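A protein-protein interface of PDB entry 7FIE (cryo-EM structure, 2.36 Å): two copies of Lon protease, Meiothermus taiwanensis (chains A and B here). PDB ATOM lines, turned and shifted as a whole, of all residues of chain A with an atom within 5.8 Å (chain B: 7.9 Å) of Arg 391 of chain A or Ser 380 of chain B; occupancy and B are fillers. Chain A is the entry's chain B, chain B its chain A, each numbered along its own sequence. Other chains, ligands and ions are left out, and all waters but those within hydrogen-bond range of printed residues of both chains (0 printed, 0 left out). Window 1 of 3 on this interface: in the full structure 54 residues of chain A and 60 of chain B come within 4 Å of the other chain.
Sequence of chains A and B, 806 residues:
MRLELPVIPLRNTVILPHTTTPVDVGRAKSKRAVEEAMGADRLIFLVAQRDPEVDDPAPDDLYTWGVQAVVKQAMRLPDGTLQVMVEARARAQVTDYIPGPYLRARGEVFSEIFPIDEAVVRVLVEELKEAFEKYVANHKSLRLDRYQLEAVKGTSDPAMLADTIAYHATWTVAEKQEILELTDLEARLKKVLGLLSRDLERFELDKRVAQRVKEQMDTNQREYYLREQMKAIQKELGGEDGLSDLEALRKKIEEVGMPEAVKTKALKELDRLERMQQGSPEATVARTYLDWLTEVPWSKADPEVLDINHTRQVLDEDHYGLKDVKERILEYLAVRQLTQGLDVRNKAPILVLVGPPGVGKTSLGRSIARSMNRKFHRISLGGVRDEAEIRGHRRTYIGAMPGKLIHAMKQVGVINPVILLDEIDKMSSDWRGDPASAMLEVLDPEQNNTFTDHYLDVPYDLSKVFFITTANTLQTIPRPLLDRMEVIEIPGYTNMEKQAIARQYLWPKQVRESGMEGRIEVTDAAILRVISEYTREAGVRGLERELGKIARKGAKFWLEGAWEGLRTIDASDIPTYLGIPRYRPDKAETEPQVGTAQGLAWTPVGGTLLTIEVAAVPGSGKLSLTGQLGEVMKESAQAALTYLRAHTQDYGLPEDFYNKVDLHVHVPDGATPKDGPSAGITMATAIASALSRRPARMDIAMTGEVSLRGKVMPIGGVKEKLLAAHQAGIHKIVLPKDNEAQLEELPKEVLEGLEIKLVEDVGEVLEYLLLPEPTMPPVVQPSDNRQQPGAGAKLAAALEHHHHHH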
ATOM      1  N   GLU A 387     -17.009  14.724  34.704  1.00  0.00           N
ATOM      2  CA  GLU A 387     -16.105  14.950  33.591  1.00  0.00           C
ATOM      3  C   GLU A 387     -16.786  15.617  32.414  1.00  0.00           C
ATOM      4  O   GLU A 387     -16.100  16.106  31.516  1.00  0.00           O
ATOM      5  CB  GLU A 387     -15.484  13.632  33.125  1.00  0.00           C
ATOM      6  CG  GLU A 387     -14.601  12.939  34.141  1.00  0.00           C
ATOM      7  CD  GLU A 387     -15.370  12.000  35.051  1.00  0.00           C
ATOM      8  OE1 GLU A 387     -16.604  11.889  34.895  1.00  0.00           O
ATOM      9  OE2 GLU A 387     -14.733  11.348  35.902  1.00  0.00           O
ATOM     10  N   ALA A 388     -18.115  15.664  32.402  1.00  0.00           N
ATOM     11  CA  ALA A 388     -18.862  16.331  31.347  1.00  0.00           C
ATOM     12  C   ALA A 388     -18.892  17.839  31.504  1.00  0.00           C
ATOM     13  O   ALA A 388     -19.599  18.510  30.752  1.00  0.00           O
ATOM     14  CB  ALA A 388     -20.295  15.800  31.292  1.00  0.00           C
ATOM     15  N   GLU A 389     -18.142  18.388  32.452  1.00  0.00           N
ATOM     16  CA  GLU A 389     -18.016  19.820  32.608  1.00  0.00           C
ATOM     17  C   GLU A 389     -16.705  20.338  32.034  1.00  0.00           C
ATOM     18  O   GLU A 389     -16.613  21.524  31.700  1.00  0.00           O
ATOM     19  CB  GLU A 389     -18.124  20.179  34.095  1.00  0.00           C
ATOM     20  CG  GLU A 389     -18.516  21.604  34.356  1.00  0.00           C
ATOM     21  CD  GLU A 389     -19.958  21.874  33.962  1.00  0.00           C
ATOM     22  OE1 GLU A 389     -20.782  20.938  34.043  1.00  0.00           O
ATOM     23  OE2 GLU A 389     -20.276  23.013  33.559  1.00  0.00           O
ATOM     24  N   ILE A 390     -15.709  19.474  31.888  1.00  0.00           N
ATOM     25  CA  ILE A 390     -14.458  19.803  31.221  1.00  0.00           C
ATOM     26  C   ILE A 390     -14.561  19.567  29.724  1.00  0.00           C
ATOM     27  O   ILE A 390     -14.421  20.494  28.930  1.00  0.00           O
ATOM     28  CB  ILE A 390     -13.304  18.983  31.837  1.00  0.00           C
ATOM     29  CG1 ILE A 390     -13.254  19.192  33.348  1.00  0.00           C
ATOM     30  CG2 ILE A 390     -11.990  19.367  31.204  1.00  0.00           C
ATOM     31  CD1 ILE A 390     -13.029  20.613  33.761  1.00  0.00           C
ATOM     32  N   ARG A 391     -14.812  18.326  29.325  1.00  0.00           N
ATOM     33  CA  ARG A 391     -15.186  17.983  27.965  1.00  0.00           C
ATOM     34  C   ARG A 391     -16.700  18.081  27.860  1.00  0.00           C
ATOM     35  O   ARG A 391     -17.399  18.240  28.858  1.00  0.00           O
ATOM     36  CB  ARG A 391     -14.712  16.574  27.595  1.00  0.00           C
ATOM     37  CG  ARG A 391     -13.208  16.385  27.648  1.00  0.00           C
ATOM     38  CD  ARG A 391     -12.828  14.994  27.190  1.00  0.00           C
ATOM     39  NE  ARG A 391     -11.397  14.732  27.264  1.00  0.00           N
ATOM     40  CZ  ARG A 391     -10.808  14.094  28.268  1.00  0.00           C
ATOM     41  NH1 ARG A 391     -11.531  13.640  29.280  1.00  0.00           N
ATOM     42  NH2 ARG A 391      -9.501  13.891  28.250  1.00  0.00           N
ATOM     43  N   GLY A 392     -17.220  18.006  26.649  1.00  0.00           N
ATOM     44  CA  GLY A 392     -18.654  18.113  26.474  1.00  0.00           C
ATOM     45  C   GLY A 392     -19.340  16.762  26.481  1.00  0.00           C
ATOM     46  O   GLY A 392     -18.833  15.757  26.976  1.00  0.00           O
ATOM     47  N   HIS A 393     -20.548  16.758  25.937  1.00  0.00           N
ATOM     48  CA  HIS A 393     -21.222  15.547  25.507  1.00  0.00           C
ATOM     49  C   HIS A 393     -21.144  15.464  23.991  1.00  0.00           C
ATOM     50  O   HIS A 393     -20.791  16.434  23.320  1.00  0.00           O
ATOM     51  CB  HIS A 393     -22.686  15.519  25.963  1.00  0.00           C
ATOM     52  CG  HIS A 393     -22.864  15.334  27.437  1.00  0.00           C
ATOM     53  ND1 HIS A 393     -22.688  14.119  28.061  1.00  0.00           N
ATOM     54  CD2 HIS A 393     -23.222  16.206  28.408  1.00  0.00           C
ATOM     55  CE1 HIS A 393     -22.919  14.252  29.354  1.00  0.00           C
ATOM     56  NE2 HIS A 393     -23.245  15.509  29.590  1.00  0.00           N
ATOM     57  N   MET A 401     -23.746  20.533  24.496  1.00  0.00           N
ATOM     58  CA  MET A 401     -22.922  21.688  24.174  1.00  0.00           C
ATOM     59  C   MET A 401     -21.547  21.428  24.790  1.00  0.00           C
ATOM     60  O   MET A 401     -21.436  20.526  25.627  1.00  0.00           O
ATOM     61  CB  MET A 401     -23.585  22.978  24.677  1.00  0.00           C
ATOM     62  CG  MET A 401     -23.583  23.216  26.165  1.00  0.00           C
ATOM     63  SD  MET A 401     -24.906  22.394  27.051  1.00  0.00           S
ATOM     64  CE  MET A 401     -24.989  23.460  28.481  1.00  0.00           C
ATOM     65  N   PRO A 402     -20.458  22.145  24.385  1.00  0.00           N
ATOM     66  CA  PRO A 402     -19.124  21.798  24.905  1.00  0.00           C
ATOM     67  C   PRO A 402     -18.905  22.078  26.382  1.00  0.00           C
ATOM     68  O   PRO A 402     -19.786  22.588  27.078  1.00  0.00           O
ATOM     69  CB  PRO A 402     -18.186  22.672  24.066  1.00  0.00           C
ATOM     70  CG  PRO A 402     -18.922  22.986  22.868  1.00  0.00           C
ATOM     71  CD  PRO A 402     -20.344  23.106  23.273  1.00  0.00           C
ATOM     72  N   GLY A 403     -17.703  21.766  26.860  1.00  0.00           N
ATOM     73  CA  GLY A 403     -17.329  22.026  28.234  1.00  0.00           C
ATOM     74  C   GLY A 403     -17.077  23.490  28.520  1.00  0.00           C
ATOM     75  O   GLY A 403     -17.326  24.349  27.672  1.00  0.00           O
ATOM     76  N   LYS A 404     -16.568  23.795  29.713  1.00  0.00           N
ATOM     77  CA  LYS A 404     -16.396  25.191  30.091  1.00  0.00           C
ATOM     78  C   LYS A 404     -15.213  25.842  29.395  1.00  0.00           C
ATOM     79  O   LYS A 404     -15.168  27.070  29.303  1.00  0.00           O
ATOM     80  CB  LYS A 404     -16.242  25.310  31.603  1.00  0.00           C
ATOM     81  CG  LYS A 404     -17.475  24.886  32.366  1.00  0.00           C
ATOM     82  CD  LYS A 404     -17.297  25.042  33.859  1.00  0.00           C
ATOM     83  CE  LYS A 404     -17.421  26.487  34.281  1.00  0.00           C
ATOM     84  NZ  LYS A 404     -18.825  26.969  34.152  1.00  0.00           N
ATOM     85  N   SER A 437      -8.399  14.077  36.298  1.00  0.00           N
ATOM     86  CA  SER A 437      -7.678  13.333  35.288  1.00  0.00           C
ATOM     87  C   SER A 437      -8.108  13.692  33.878  1.00  0.00           C
ATOM     88  O   SER A 437      -7.509  13.198  32.923  1.00  0.00           O
ATOM     89  CB  SER A 437      -7.855  11.830  35.512  1.00  0.00           C
ATOM     90  OG  SER A 437      -9.201  11.455  35.322  1.00  0.00           O
ATOM     91  N   ALA A 438      -9.129  14.526  33.729  1.00  0.00           N
ATOM     92  CA  ALA A 438      -9.450  15.139  32.453  1.00  0.00           C
ATOM     93  C   ALA A 438      -8.823  16.512  32.297  1.00  0.00           C
ATOM     94  O   ALA A 438      -8.796  17.038  31.182  1.00  0.00           O
ATOM     95  CB  ALA A 438     -10.962  15.251  32.279  1.00  0.00           C
ATOM     96  N   LEU A 440      -5.689  16.794  32.852  1.00  0.00           N
ATOM     97  CA  LEU A 440      -4.572  16.342  32.044  1.00  0.00           C
ATOM     98  C   LEU A 440      -5.005  16.487  30.594  1.00  0.00           C
ATOM     99  O   LEU A 440      -6.170  16.238  30.285  1.00  0.00           O
ATOM    100  CB  LEU A 440      -4.233  14.892  32.375  1.00  0.00           C
ATOM    101  CG  LEU A 440      -3.959  14.583  33.845  1.00  0.00           C
ATOM    102  CD1 LEU A 440      -3.764  13.105  34.039  1.00  0.00           C
ATOM    103  CD2 LEU A 440      -2.771  15.338  34.355  1.00  0.00           C
ATOM    104  N   GLU A 441      -4.075  16.917  29.738  1.00  0.00           N
ATOM    105  CA  GLU A 441      -4.142  17.341  28.327  1.00  0.00           C
ATOM    106  C   GLU A 441      -4.797  18.707  28.159  1.00  0.00           C
ATOM    107  O   GLU A 441      -4.750  19.289  27.070  1.00  0.00           O
ATOM    108  CB  GLU A 441      -4.843  16.355  27.371  1.00  0.00           C
ATOM    109  CG  GLU A 441      -6.360  16.487  27.202  1.00  0.00           C
ATOM    110  CD  GLU A 441      -6.895  15.629  26.085  1.00  0.00           C
ATOM    111  OE1 GLU A 441      -6.078  15.002  25.384  1.00  0.00           O
ATOM    112  OE2 GLU A 441      -8.129  15.580  25.899  1.00  0.00           O
ATOM    113  N   PHE A 451      -5.785  19.569  21.921  1.00  0.00           N
ATOM    114  CA  PHE A 451      -6.862  19.273  22.856  1.00  0.00           C
ATOM    115  C   PHE A 451      -8.150  18.999  22.099  1.00  0.00           C
ATOM    116  O   PHE A 451      -8.593  19.819  21.290  1.00  0.00           O
ATOM    117  CB  PHE A 451      -7.064  20.428  23.831  1.00  0.00           C
ATOM    118  CG  PHE A 451      -8.269  20.271  24.709  1.00  0.00           C
ATOM    119  CD1 PHE A 451      -8.286  19.332  25.720  1.00  0.00           C
ATOM    120  CD2 PHE A 451      -9.386  21.071  24.527  1.00  0.00           C
ATOM    121  CE1 PHE A 451      -9.395  19.182  26.523  1.00  0.00           C
ATOM    122  CE2 PHE A 451     -10.496  20.926  25.331  1.00  0.00           C
ATOM    123  CZ  PHE A 451     -10.499  19.982  26.328  1.00  0.00           C
ATOM    124  N   THR A 452      -8.754  17.849  22.363  1.00  0.00           N
ATOM    125  CA  THR A 452      -9.959  17.427  21.664  1.00  0.00           C
ATOM    126  C   THR A 452     -11.139  17.419  22.630  1.00  0.00           C
ATOM    127  O   THR A 452     -11.046  16.896  23.745  1.00  0.00           O
ATOM    128  CB  THR A 452      -9.751  16.069  20.982  1.00  0.00           C
ATOM    129  OG1 THR A 452     -10.966  15.642  20.355  1.00  0.00           O
ATOM    130  CG2 THR A 452      -9.226  14.996  21.934  1.00  0.00           C
ATOM    131  N   ASP A 453     -12.225  18.057  22.217  1.00  0.00           N
ATOM    132  CA  ASP A 453     -13.460  18.091  22.977  1.00  0.00           C
ATOM    133  C   ASP A 453     -14.300  16.877  22.585  1.00  0.00           C
ATOM    134  O   ASP A 453     -13.940  16.111  21.693  1.00  0.00           O
ATOM    135  CB  ASP A 453     -14.186  19.414  22.705  1.00  0.00           C
ATOM    136  CG  ASP A 453     -15.240  19.743  23.744  1.00  0.00           C
ATOM    137  OD1 ASP A 453     -14.869  20.136  24.866  1.00  0.00           O
ATOM    138  OD2 ASP A 453     -16.439  19.610  23.435  1.00  0.00           O
ATOM    139  N   HIS A 454     -15.416  16.675  23.279  1.00  0.00           N
ATOM    140  CA  HIS A 454     -16.366  15.653  22.876  1.00  0.00           C
ATOM    141  C   HIS A 454     -17.512  16.194  22.039  1.00  0.00           C
ATOM    142  O   HIS A 454     -18.122  15.424  21.292  1.00  0.00           O
ATOM    143  CB  HIS A 454     -16.928  14.921  24.101  1.00  0.00           C
ATOM    144  CG  HIS A 454     -15.965  13.962  24.724  1.00  0.00           C
ATOM    145  ND1 HIS A 454     -16.223  13.319  25.914  1.00  0.00           N
ATOM    146  CD2 HIS A 454     -14.749  13.531  24.320  1.00  0.00           C
ATOM    147  CE1 HIS A 454     -15.206  12.533  26.217  1.00  0.00           C
ATOM    148  NE2 HIS A 454     -14.298  12.644  25.265  1.00  0.00           N
ATOM    149  N   HIS B 377      -1.288   8.043  15.836  1.00  0.00           N
ATOM    150  CA  HIS B 377      -2.478   8.732  16.304  1.00  0.00           C
ATOM    151  C   HIS B 377      -2.637   8.462  17.790  1.00  0.00           C
ATOM    152  O   HIS B 377      -2.529   7.317  18.229  1.00  0.00           O
ATOM    153  CB  HIS B 377      -3.723   8.280  15.542  1.00  0.00           C
ATOM    154  CG  HIS B 377      -4.939   9.094  15.839  1.00  0.00           C
ATOM    155  ND1 HIS B 377      -5.779   8.816  16.894  1.00  0.00           N
ATOM    156  CD2 HIS B 377      -5.459  10.177  15.218  1.00  0.00           C
ATOM    157  CE1 HIS B 377      -6.764   9.696  16.911  1.00  0.00           C
ATOM    158  NE2 HIS B 377      -6.594  10.532  15.904  1.00  0.00           N
ATOM    159  N   ARG B 378      -2.893   9.513  18.560  1.00  0.00           N
ATOM    160  CA  ARG B 378      -2.964   9.421  20.010  1.00  0.00           C
ATOM    161  C   ARG B 378      -4.397   9.627  20.470  1.00  0.00           C
ATOM    162  O   ARG B 378      -5.077  10.544  20.002  1.00  0.00           O
ATOM    163  CB  ARG B 378      -2.048  10.452  20.665  1.00  0.00           C
ATOM    164  CG  ARG B 378      -1.953  10.331  22.167  1.00  0.00           C
ATOM    165  CD  ARG B 378      -0.980  11.340  22.722  1.00  0.00           C
ATOM    166  NE  ARG B 378      -1.443  12.704  22.525  1.00  0.00           N
ATOM    167  CZ  ARG B 378      -2.215  13.354  23.385  1.00  0.00           C
ATOM    168  NH1 ARG B 378      -2.584  12.772  24.514  1.00  0.00           N
ATOM    169  NH2 ARG B 378      -2.596  14.594  23.124  1.00  0.00           N
ATOM    170  N   ILE B 379      -4.850   8.775  21.383  1.00  0.00           N
ATOM    171  CA  ILE B 379      -6.188   8.852  21.954  1.00  0.00           C
ATOM    172  C   ILE B 379      -6.040   8.979  23.459  1.00  0.00           C
ATOM    173  O   ILE B 379      -5.415   8.126  24.099  1.00  0.00           O
ATOM    174  CB  ILE B 379      -7.036   7.625  21.592  1.00  0.00           C
ATOM    175  CG1 ILE B 379      -7.264   7.551  20.088  1.00  0.00           C
ATOM    176  CG2 ILE B 379      -8.360   7.664  22.309  1.00  0.00           C
ATOM    177  CD1 ILE B 379      -7.888   6.261  19.651  1.00  0.00           C
ATOM    178  N   SER B 380      -6.609  10.033  24.026  1.00  0.00           N
ATOM    179  CA  SER B 380      -6.516  10.266  25.458  1.00  0.00           C
ATOM    180  C   SER B 380      -7.739   9.695  26.157  1.00  0.00           C
ATOM    181  O   SER B 380      -8.874  10.011  25.794  1.00  0.00           O
ATOM    182  CB  SER B 380      -6.393  11.755  25.756  1.00  0.00           C
ATOM    183  OG  SER B 380      -6.305  11.976  27.148  1.00  0.00           O
ATOM    184  N   LEU B 381      -7.501   8.859  27.164  1.00  0.00           N
ATOM    185  CA  LEU B 381      -8.564   8.177  27.885  1.00  0.00           C
ATOM    186  C   LEU B 381      -8.652   8.619  29.335  1.00  0.00           C
ATOM    187  O   LEU B 381      -9.138   7.862  30.177  1.00  0.00           O
ATOM    188  CB  LEU B 381      -8.354   6.667  27.816  1.00  0.00           C
ATOM    189  CG  LEU B 381      -8.451   6.033  26.436  1.00  0.00           C
ATOM    190  CD1 LEU B 381      -8.019   4.595  26.515  1.00  0.00           C
ATOM    191  CD2 LEU B 381      -9.858   6.137  25.894  1.00  0.00           C
ATOM    192  N   GLY B 382      -8.202   9.829  29.641  1.00  0.00           N
ATOM    193  CA  GLY B 382      -8.027  10.293  30.996  1.00  0.00           C
ATOM    194  C   GLY B 382      -9.275  10.460  31.823  1.00  0.00           C
ATOM    195  O   GLY B 382      -9.233  10.240  33.033  1.00  0.00           O
ATOM    196  N   GLY B 383     -10.395  10.832  31.229  1.00  0.00           N
ATOM    197  CA  GLY B 383     -11.598  10.988  32.015  1.00  0.00           C
ATOM    198  C   GLY B 383     -12.818  10.487  31.284  1.00  0.00           C
ATOM    199  O   GLY B 383     -13.926  10.977  31.511  1.00  0.00           O
ATOM    200  N   VAL B 384     -12.619   9.526  30.390  1.00  0.00           N
ATOM    201  CA  VAL B 384     -13.696   9.002  29.562  1.00  0.00           C
ATOM    202  C   VAL B 384     -14.622   8.183  30.445  1.00  0.00           C
ATOM    203  O   VAL B 384     -14.185   7.251  31.127  1.00  0.00           O
ATOM    204  CB  VAL B 384     -13.150   8.164  28.400  1.00  0.00           C
ATOM    205  CG1 VAL B 384     -14.290   7.575  27.601  1.00  0.00           C
ATOM    206  CG2 VAL B 384     -12.276   9.017  27.510  1.00  0.00           C
ATOM    207  N   ARG B 385     -15.900   8.544  30.440  1.00  0.00           N
ATOM    208  CA  ARG B 385     -16.893   7.914  31.286  1.00  0.00           C
ATOM    209  C   ARG B 385     -17.914   7.114  30.498  1.00  0.00           C
ATOM    210  O   ARG B 385     -18.351   6.061  30.971  1.00  0.00           O
ATOM    211  CB  ARG B 385     -17.620   8.981  32.122  1.00  0.00           C
ATOM    212  CG  ARG B 385     -18.506   8.438  33.219  1.00  0.00           C
ATOM    213  CD  ARG B 385     -19.167   9.546  34.021  1.00  0.00           C
ATOM    214  NE  ARG B 385     -20.122  10.310  33.224  1.00  0.00           N
ATOM    215  CZ  ARG B 385     -19.994  11.600  32.939  1.00  0.00           C
ATOM    216  NH1 ARG B 385     -18.952  12.279  33.391  1.00  0.00           N
ATOM    217  NH2 ARG B 385     -20.912  12.214  32.208  1.00  0.00           N
ATOM    218  N   GLU B 389     -17.981   6.307  23.455  1.00  0.00           N
ATOM    219  CA  GLU B 389     -16.792   6.851  22.823  1.00  0.00           C
ATOM    220  C   GLU B 389     -15.970   5.763  22.160  1.00  0.00           C
ATOM    221  O   GLU B 389     -15.367   6.005  21.111  1.00  0.00           O
ATOM    222  CB  GLU B 389     -15.927   7.578  23.853  1.00  0.00           C
ATOM    223  CG  GLU B 389     -16.571   8.781  24.486  1.00  0.00           C
ATOM    224  CD  GLU B 389     -16.754   9.920  23.521  1.00  0.00           C
ATOM    225  OE1 GLU B 389     -15.935  10.073  22.589  1.00  0.00           O
ATOM    226  OE2 GLU B 389     -17.722  10.679  23.703  1.00  0.00           O
ATOM    227  N   ILE B 390     -15.964   4.561  22.726  1.00  0.00           N
ATOM    228  CA  ILE B 390     -15.228   3.439  22.174  1.00  0.00           C
ATOM    229  C   ILE B 390     -15.996   2.780  21.038  1.00  0.00           C
ATOM    230  O   ILE B 390     -15.518   2.726  19.905  1.00  0.00           O
ATOM    231  CB  ILE B 390     -14.896   2.411  23.274  1.00  0.00           C
ATOM    232  CG1 ILE B 390     -14.234   3.102  24.468  1.00  0.00           C
ATOM    233  CG2 ILE B 390     -14.030   1.307  22.712  1.00  0.00           C
ATOM    234  CD1 ILE B 390     -12.987   3.892  24.128  1.00  0.00           C
ATOM    235  N   LYS B 404     -14.450   6.235  18.680  1.00  0.00           N
ATOM    236  CA  LYS B 404     -13.197   6.960  18.495  1.00  0.00           C
ATOM    237  C   LYS B 404     -12.151   6.109  17.791  1.00  0.00           C
ATOM    238  O   LYS B 404     -11.264   6.653  17.128  1.00  0.00           O
ATOM    239  CB  LYS B 404     -12.657   7.447  19.839  1.00  0.00           C
ATOM    240  CG  LYS B 404     -13.443   8.587  20.461  1.00  0.00           C
ATOM    241  CD  LYS B 404     -12.929   8.916  21.854  1.00  0.00           C
ATOM    242  CE  LYS B 404     -11.609   9.649  21.811  1.00  0.00           C
ATOM    243  NZ  LYS B 404     -11.781  11.022  21.268  1.00  0.00           N
ATOM    244  N   LEU B 420      -1.634   5.177  20.242  1.00  0.00           N
ATOM    245  CA  LEU B 420      -1.230   5.384  21.626  1.00  0.00           C
ATOM    246  C   LEU B 420      -2.479   5.636  22.457  1.00  0.00           C
ATOM    247  O   LEU B 420      -3.127   6.675  22.310  1.00  0.00           O
ATOM    248  CB  LEU B 420      -0.265   6.556  21.736  1.00  0.00           C
ATOM    249  CG  LEU B 420       0.215   6.875  23.146  1.00  0.00           C
ATOM    250  CD1 LEU B 420       1.059   5.759  23.678  1.00  0.00           C
ATOM    251  CD2 LEU B 420       0.983   8.164  23.165  1.00  0.00           C
ATOM    252  N   LEU B 421      -2.817   4.690  23.326  1.00  0.00           N
ATOM    253  CA  LEU B 421      -3.938   4.846  24.249  1.00  0.00           C
ATOM    254  C   LEU B 421      -3.378   5.372  25.558  1.00  0.00           C
ATOM    255  O   LEU B 421      -2.769   4.630  26.327  1.00  0.00           O
ATOM    256  CB  LEU B 421      -4.665   3.524  24.451  1.00  0.00           C
ATOM    257  CG  LEU B 421      -5.348   2.958  23.216  1.00  0.00           C
ATOM    258  CD1 LEU B 421      -5.913   1.596  23.525  1.00  0.00           C
ATOM    259  CD2 LEU B 421      -6.430   3.896  22.749  1.00  0.00           C
ATOM    260  N   ASP B 422      -3.582   6.652  25.822  1.00  0.00           N
ATOM    261  CA  ASP B 422      -2.890   7.308  26.916  1.00  0.00           C
ATOM    262  C   ASP B 422      -3.757   7.283  28.168  1.00  0.00           C
ATOM    263  O   ASP B 422      -4.966   7.517  28.093  1.00  0.00           O
ATOM    264  CB  ASP B 422      -2.541   8.742  26.528  1.00  0.00           C
ATOM    265  CG  ASP B 422      -1.408   9.304  27.344  1.00  0.00           C
ATOM    266  OD1 ASP B 422      -0.891   8.584  28.218  1.00  0.00           O
ATOM    267  OD2 ASP B 422      -1.018  10.463  27.102  1.00  0.00           O
ATOM    268  N   GLU B 423      -3.125   6.986  29.308  1.00  0.00           N
ATOM    269  CA  GLU B 423      -3.734   6.910  30.634  1.00  0.00           C
ATOM    270  C   GLU B 423      -4.896   5.928  30.705  1.00  0.00           C
ATOM    271  O   GLU B 423      -6.036   6.331  30.944  1.00  0.00           O
ATOM    272  CB  GLU B 423      -4.197   8.292  31.102  1.00  0.00           C
ATOM    273  CG  GLU B 423      -3.082   9.310  31.243  1.00  0.00           C
ATOM    274  CD  GLU B 423      -2.092   8.960  32.338  1.00  0.00           C
ATOM    275  OE1 GLU B 423      -2.498   8.351  33.349  1.00  0.00           O
ATOM    276  OE2 GLU B 423      -0.900   9.298  32.187  1.00  0.00           O
ATOM    277  N   ILE B 424      -4.625   4.641  30.500  1.00  0.00           N
ATOM    278  CA  ILE B 424      -5.661   3.617  30.588  1.00  0.00           C
ATOM    279  C   ILE B 424      -6.009   3.300  32.035  1.00  0.00           C
ATOM    280  O   ILE B 424      -7.043   2.684  32.310  1.00  0.00           O
ATOM    281  CB  ILE B 424      -5.247   2.342  29.829  1.00  0.00           C
ATOM    282  CG1 ILE B 424      -3.793   1.962  30.124  1.00  0.00           C
ATOM    283  CG2 ILE B 424      -5.486   2.502  28.349  1.00  0.00           C
ATOM    284  CD1 ILE B 424      -3.584   0.994  31.248  1.00  0.00           C
ATOM    285  N   MET B 427      -9.559   5.542  33.507  1.00  0.00           N
ATOM    286  CA  MET B 427     -10.906   5.580  32.959  1.00  0.00           C
ATOM    287  C   MET B 427     -11.927   5.548  34.086  1.00  0.00           C
ATOM    288  O   MET B 427     -11.727   4.874  35.099  1.00  0.00           O
ATOM    289  CB  MET B 427     -11.131   4.407  32.014  1.00  0.00           C
ATOM    290  CG  MET B 427     -10.336   4.480  30.736  1.00  0.00           C
ATOM    291  SD  MET B 427     -10.710   3.102  29.648  1.00  0.00           S
ATOM    292  CE  MET B 427      -9.842   1.784  30.486  1.00  0.00           C
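Arg 391 of chain A touches just these residues of chain B: Ser 380 and Gly 383.
Gly 392 of chain A touches none of the printed residues of chain B.
Printed residues of chain B within 4 Å of His 454 of chain A: Glu 389.
Ser 380 of chain B touches just these residues of chain A: Arg 391 and Glu 441.
Of the printed residues of chain A, Gly 383 of chain B touches Glu 387 (3.3 Å) and Arg 391 (3.6 Å).
Printed residues of chain A within 4 Å of Glu 389 of chain B: His 454 (3.8 Å).
The nearest residue of chain A that does not touch Ser 380 of chain B is Leu 440 of chain A (5.3 Å).
Among the printed residues, Asp or Glu carboxylates within 4 Å of a Lys or Arg side-chain nitrogen of the other chain: Glu 387 of chain A with Arg 385 of chain B (2.8 Å).
OE1 of Glu 387 of chain A is in salt-bridge range of NH1 of Arg 385 of chain B (2.8 Å).
The backbone carbonyl oxygen (O) of Gly 382 of chain B lies within hydrogen-bond range of the side-chain hydroxyl (OG) of Ser 437 of chain A, at 2.6 Å.
Positions printed for both chains: 389, 390 and 404.
Gly 383 of chain B touches Glu 387 of chain A (O to CG, 3.3 Å).
Arg 385 of chain B touches Ala 388 of chain A.
Arg 391 of chain A touches Ser 380 of chain B (NH2 to OG, 3.9 Å).
NH1 of Arg 391 of chain A touches N of Gly 383 of chain B, at 3.6 Å.
Ser 380 of chain B touches Glu 441 of chain A (CB to OE1, 3.3 Å).
ND1 of His 454 of chain A touches OE2 of Glu 389 of chain B, at 3.8 Å.
The guanidinium group (NH2) of Arg 391 of chain A lies within salt-bridge range of the side-chain carboxylate (OE2) of Glu 441 of chain A (3.2 Å).
O of Glu 389 of chain B lies within hydrogen-bond range of N of Lys 404 of chain B (2.6 Å).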
